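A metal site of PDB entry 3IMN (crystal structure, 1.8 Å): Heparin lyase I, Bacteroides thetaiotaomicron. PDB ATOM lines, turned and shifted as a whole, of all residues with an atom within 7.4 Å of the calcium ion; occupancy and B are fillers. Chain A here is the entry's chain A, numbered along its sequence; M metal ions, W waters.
Water W1 lies within hydrogen-bond range of the backbone carbonyl oxygen (O) of Lys 247 (2.6 Å) and the side-chain hydroxyl (OG1) of Thr 250 (2.9 Å).
The calcium ion is bound by the backbone carbonyl oxygen (O) of Trp 248 (2.4 Å), the side-chain carboxylate (OD1) of Asp 346 (2.4 Å), water W1 (2.5 Å), the side-chain carboxylate (OE2) of Glu 222 (2.5 Å), the backbone carbonyl oxygen (O) of Asn 345 (2.6 Å) and the side-chain carboxylate (OE1) of Glu 222 (2.8 Å).
The calcium ion has six donor atoms within binding distance.
The side-chain carboxylate (OE1) of Glu 222 sits close to the backbone NH (N) of Asp 155 (2.7 Å).
O of Leu 158 lies within hydrogen-bond range of N of Glu 222 (3.3 Å).
The guanidinium group of Arg 344 is in salt-bridge range of the side-chain carboxylate of Asp 346 (2.5 Å).
The side-chain carboxylate (OE1) of Glu 222 lies close to the guanidinium group (NH2) of Arg 344, at 3.5 Å.
ND2 of Asn 345 sits at hydrogen-bond distance from O of Arg 246, at 2.8 Å.
N of Asn 345 sits at hydrogen-bond distance from O of Asp 245, at 2.8 Å.
N of Glu 347 sits at hydrogen-bond distance from OD2 of Asp 155 (2.9 Å).
The backbone NH (N) of Thr 250 lies close to the side-chain carboxylate (OE2) of Glu 222.
Merely in contact with the calcium ion: Asp 155 (3.9 Å).
The nearest printed residue that does not touch the calcium ion is Lys 247 (4.02 Å).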
ATOM      1  N   MET A 153      -7.276 -18.256  -3.896  1.00  0.00           N
ATOM      2  CA  MET A 153      -8.546 -18.013  -3.212  1.00  0.00           C
ATOM      3  C   MET A 153      -8.535 -18.949  -1.975  1.00  0.00           C
ATOM      4  O   MET A 153      -8.880 -20.111  -2.082  1.00  0.00           O
ATOM      5  CB  MET A 153      -9.686 -18.375  -4.184  1.00  0.00           C
ATOM      6  CG  MET A 153      -9.731 -17.386  -5.377  1.00  0.00           C
ATOM      7  SD  MET A 153     -10.938 -17.935  -6.613  1.00  0.00           S
ATOM      8  CE  MET A 153     -12.329 -17.191  -5.856  1.00  0.00           C
ATOM      9  N   PRO A 154      -8.087 -18.436  -0.823  1.00  0.00           N
ATOM     10  CA  PRO A 154      -7.901 -19.341   0.341  1.00  0.00           C
ATOM     11  C   PRO A 154      -9.178 -19.942   0.864  1.00  0.00           C
ATOM     12  O   PRO A 154     -10.231 -19.331   0.693  1.00  0.00           O
ATOM     13  CB  PRO A 154      -7.266 -18.445   1.388  1.00  0.00           C
ATOM     14  CG  PRO A 154      -6.569 -17.316   0.556  1.00  0.00           C
ATOM     15  CD  PRO A 154      -7.497 -17.109  -0.635  1.00  0.00           C
ATOM     16  N   ASP A 155      -9.078 -21.159   1.450  1.00  0.00           N
ATOM     17  CA  ASP A 155     -10.214 -21.813   2.063  1.00  0.00           C
ATOM     18  C   ASP A 155     -10.619 -21.018   3.309  1.00  0.00           C
ATOM     19  O   ASP A 155      -9.974 -21.128   4.360  1.00  0.00           O
ATOM     20  CB  ASP A 155      -9.845 -23.240   2.523  1.00  0.00           C
ATOM     21  CG  ASP A 155      -9.609 -24.232   1.337  1.00  0.00           C
ATOM     22  OD1 ASP A 155      -9.222 -25.403   1.625  1.00  0.00           O
ATOM     23  OD2 ASP A 155      -9.829 -23.924   0.150  1.00  0.00           O
ATOM     24  N   LEU A 158     -11.390 -23.057   6.533  1.00  0.00           N
ATOM     25  CA  LEU A 158     -10.368 -24.004   6.963  1.00  0.00           C
ATOM     26  C   LEU A 158      -9.607 -23.433   8.146  1.00  0.00           C
ATOM     27  O   LEU A 158      -8.969 -22.371   8.045  1.00  0.00           O
ATOM     28  CB  LEU A 158      -9.418 -24.372   5.820  1.00  0.00           C
ATOM     29  CG  LEU A 158      -8.367 -25.475   6.064  1.00  0.00           C
ATOM     30  CD1 LEU A 158      -9.047 -26.821   6.335  1.00  0.00           C
ATOM     31  CD2 LEU A 158      -7.412 -25.603   4.908  1.00  0.00           C
ATOM     32  N   GLU A 222      -6.830 -19.953   7.264  1.00  0.00           N
ATOM     33  CA  GLU A 222      -6.049 -19.670   6.043  1.00  0.00           C
ATOM     34  C   GLU A 222      -6.333 -18.233   5.541  1.00  0.00           C
ATOM     35  O   GLU A 222      -7.492 -17.900   5.355  1.00  0.00           O
ATOM     36  CB  GLU A 222      -6.504 -20.642   4.959  1.00  0.00           C
ATOM     37  CG  GLU A 222      -5.605 -20.645   3.853  1.00  0.00           C
ATOM     38  CD  GLU A 222      -5.684 -21.886   3.060  1.00  0.00           C
ATOM     39  OE1 GLU A 222      -6.661 -22.035   2.311  1.00  0.00           O
ATOM     40  OE2 GLU A 222      -4.728 -22.699   3.151  1.00  0.00           O
ATOM     41  N   ASP A 245       2.301 -23.714  -3.141  1.00  0.00           N
ATOM     42  CA  ASP A 245       2.142 -23.997  -1.750  1.00  0.00           C
ATOM     43  C   ASP A 245       1.288 -25.306  -1.691  1.00  0.00           C
ATOM     44  O   ASP A 245       0.104 -25.305  -2.095  1.00  0.00           O
ATOM     45  CB  ASP A 245       1.436 -22.851  -1.044  1.00  0.00           C
ATOM     46  CG  ASP A 245       1.319 -23.082   0.459  1.00  0.00           C
ATOM     47  OD1 ASP A 245       1.738 -24.168   0.998  1.00  0.00           O
ATOM     48  OD2 ASP A 245       0.814 -22.173   1.110  1.00  0.00           O
ATOM     49  N   ARG A 246       1.886 -26.430  -1.242  1.00  0.00           N
ATOM     50  CA  ARG A 246       1.050 -27.663  -1.242  1.00  0.00           C
ATOM     51  C   ARG A 246       0.494 -28.022   0.139  1.00  0.00           C
ATOM     52  O   ARG A 246      -0.254 -29.041   0.293  1.00  0.00           O
ATOM     53  CB  ARG A 246       1.807 -28.840  -1.821  1.00  0.00           C
ATOM     54  CG  ARG A 246       2.914 -29.324  -0.889  1.00  0.00           C
ATOM     55  CD  ARG A 246       3.757 -30.410  -1.714  1.00  0.00           C
ATOM     56  NE  ARG A 246       5.006 -30.656  -1.023  1.00  0.00           N
ATOM     57  CZ  ARG A 246       5.224 -31.681  -0.182  1.00  0.00           C
ATOM     58  NH1 ARG A 246       4.301 -32.627   0.001  1.00  0.00           N
ATOM     59  NH2 ARG A 246       6.423 -31.830   0.353  1.00  0.00           N
ATOM     60  N   LYS A 247       0.802 -27.203   1.155  1.00  0.00           N
ATOM     61  CA  LYS A 247       0.183 -27.365   2.454  1.00  0.00           C
ATOM     62  C   LYS A 247      -1.363 -27.167   2.386  1.00  0.00           C
ATOM     63  O   LYS A 247      -1.897 -26.231   1.747  1.00  0.00           O
ATOM     64  CB  LYS A 247       0.801 -26.401   3.461  1.00  0.00           C
ATOM     65  CG  LYS A 247       1.006 -27.052   4.860  1.00  0.00           C
ATOM     66  CD  LYS A 247       1.528 -26.123   5.963  1.00  0.00           C
ATOM     67  CE  LYS A 247       1.941 -27.004   7.221  1.00  0.00           C
ATOM     68  NZ  LYS A 247       2.337 -26.133   8.351  1.00  0.00           N
ATOM     69  N   TRP A 248      -2.102 -28.023   3.091  1.00  0.00           N
ATOM     70  CA  TRP A 248      -3.552 -27.913   3.066  1.00  0.00           C
ATOM     71  C   TRP A 248      -3.956 -26.634   3.753  1.00  0.00           C
ATOM     72  O   TRP A 248      -4.703 -25.841   3.175  1.00  0.00           O
ATOM     73  CB  TRP A 248      -4.170 -29.130   3.735  1.00  0.00           C
ATOM     74  CG  TRP A 248      -5.660 -29.207   3.731  1.00  0.00           C
ATOM     75  CD1 TRP A 248      -6.475 -29.520   4.810  1.00  0.00           C
ATOM     76  CD2 TRP A 248      -6.555 -29.035   2.598  1.00  0.00           C
ATOM     77  NE1 TRP A 248      -7.796 -29.525   4.418  1.00  0.00           N
ATOM     78  CE2 TRP A 248      -7.879 -29.229   3.081  1.00  0.00           C
ATOM     79  CE3 TRP A 248      -6.363 -28.726   1.251  1.00  0.00           C
ATOM     80  CZ2 TRP A 248      -8.989 -29.120   2.257  1.00  0.00           C
ATOM     81  CZ3 TRP A 248      -7.468 -28.642   0.417  1.00  0.00           C
ATOM     82  CH2 TRP A 248      -8.783 -28.859   0.939  1.00  0.00           C
ATOM     83  N   LEU A 249      -3.460 -26.418   4.960  1.00  0.00           N
ATOM     84  CA  LEU A 249      -3.616 -25.139   5.603  1.00  0.00           C
ATOM     85  C   LEU A 249      -2.323 -24.342   5.447  1.00  0.00           C
ATOM     86  O   LEU A 249      -1.343 -24.669   6.069  1.00  0.00           O
ATOM     87  CB  LEU A 249      -3.930 -25.313   7.092  1.00  0.00           C
ATOM     88  CG  LEU A 249      -4.316 -24.069   7.901  1.00  0.00           C
ATOM     89  CD1 LEU A 249      -5.397 -23.192   7.210  1.00  0.00           C
ATOM     90  CD2 LEU A 249      -4.704 -24.389   9.338  1.00  0.00           C
ATOM     91  N   THR A 250      -2.325 -23.270   4.660  1.00  0.00           N
ATOM     92  CA  THR A 250      -1.073 -22.476   4.495  1.00  0.00           C
ATOM     93  C   THR A 250      -0.386 -22.005   5.788  1.00  0.00           C
ATOM     94  O   THR A 250      -1.032 -21.468   6.701  1.00  0.00           O
ATOM     95  CB  THR A 250      -1.302 -21.228   3.565  1.00  0.00           C
ATOM     96  OG1 THR A 250      -1.552 -21.748   2.259  1.00  0.00           O
ATOM     97  CG2 THR A 250      -0.006 -20.349   3.474  1.00  0.00           C
ATOM     98  N   ARG A 344      -1.866 -23.230  -5.503  1.00  0.00           N
ATOM     99  CA  ARG A 344      -1.983 -23.399  -4.088  1.00  0.00           C
ATOM    100  C   ARG A 344      -2.926 -24.608  -3.829  1.00  0.00           C
ATOM    101  O   ARG A 344      -3.856 -24.807  -4.566  1.00  0.00           O
ATOM    102  CB  ARG A 344      -2.759 -22.181  -3.490  1.00  0.00           C
ATOM    103  CG  ARG A 344      -2.018 -20.916  -3.385  1.00  0.00           C
ATOM    104  CD  ARG A 344      -2.969 -19.825  -2.942  1.00  0.00           C
ATOM    105  NE  ARG A 344      -3.741 -20.276  -1.779  1.00  0.00           N
ATOM    106  CZ  ARG A 344      -3.413 -20.019  -0.501  1.00  0.00           C
ATOM    107  NH1 ARG A 344      -2.325 -19.317  -0.193  1.00  0.00           N
ATOM    108  NH2 ARG A 344      -4.168 -20.467   0.499  1.00  0.00           N
ATOM    109  N   ASN A 345      -2.624 -25.393  -2.784  1.00  0.00           N
ATOM    110  CA  ASN A 345      -3.532 -26.538  -2.459  1.00  0.00           C
ATOM    111  C   ASN A 345      -4.756 -26.044  -1.720  1.00  0.00           C
ATOM    112  O   ASN A 345      -4.792 -26.003  -0.508  1.00  0.00           O
ATOM    113  CB  ASN A 345      -2.702 -27.530  -1.639  1.00  0.00           C
ATOM    114  CG  ASN A 345      -3.501 -28.760  -1.215  1.00  0.00           C
ATOM    115  OD1 ASN A 345      -4.559 -29.053  -1.790  1.00  0.00           O
ATOM    116  ND2 ASN A 345      -2.976 -29.499  -0.223  1.00  0.00           N
ATOM    117  N   ASP A 346      -5.795 -25.620  -2.503  1.00  0.00           N
ATOM    118  CA  ASP A 346      -7.038 -25.063  -1.937  1.00  0.00           C
ATOM    119  C   ASP A 346      -8.154 -25.759  -2.704  1.00  0.00           C
ATOM    120  O   ASP A 346      -7.942 -26.428  -3.709  1.00  0.00           O
ATOM    121  CB  ASP A 346      -7.231 -23.543  -2.288  1.00  0.00           C
ATOM    122  CG  ASP A 346      -6.271 -22.616  -1.523  1.00  0.00           C
ATOM    123  OD1 ASP A 346      -5.793 -22.959  -0.420  1.00  0.00           O
ATOM    124  OD2 ASP A 346      -5.963 -21.476  -1.980  1.00  0.00           O
ATOM    125  N   GLU A 347      -9.371 -25.489  -2.259  1.00  0.00           N
ATOM    126  CA  GLU A 347     -10.580 -25.988  -2.942  1.00  0.00           C
ATOM    127  C   GLU A 347     -10.820 -25.155  -4.180  1.00  0.00           C
ATOM    128  O   GLU A 347     -11.090 -25.698  -5.243  1.00  0.00           O
ATOM    129  CB  GLU A 347     -11.821 -25.825  -2.025  1.00  0.00           C
ATOM    130  CG  GLU A 347     -12.818 -26.887  -2.434  1.00  0.00           C
ATOM    131  CD  GLU A 347     -12.240 -28.319  -2.147  1.00  0.00           C
ATOM    132  OE1 GLU A 347     -12.049 -28.695  -0.960  1.00  0.00           O
ATOM    133  OE2 GLU A 347     -11.986 -29.074  -3.117  1.00  0.00           O
HETATM  134 CA    CA M   1      -5.470 -24.402   1.455  1.00  0.00          CA
HETATM  135  O   HOH W   1      -3.073 -23.951   1.129  1.00  0.00           O
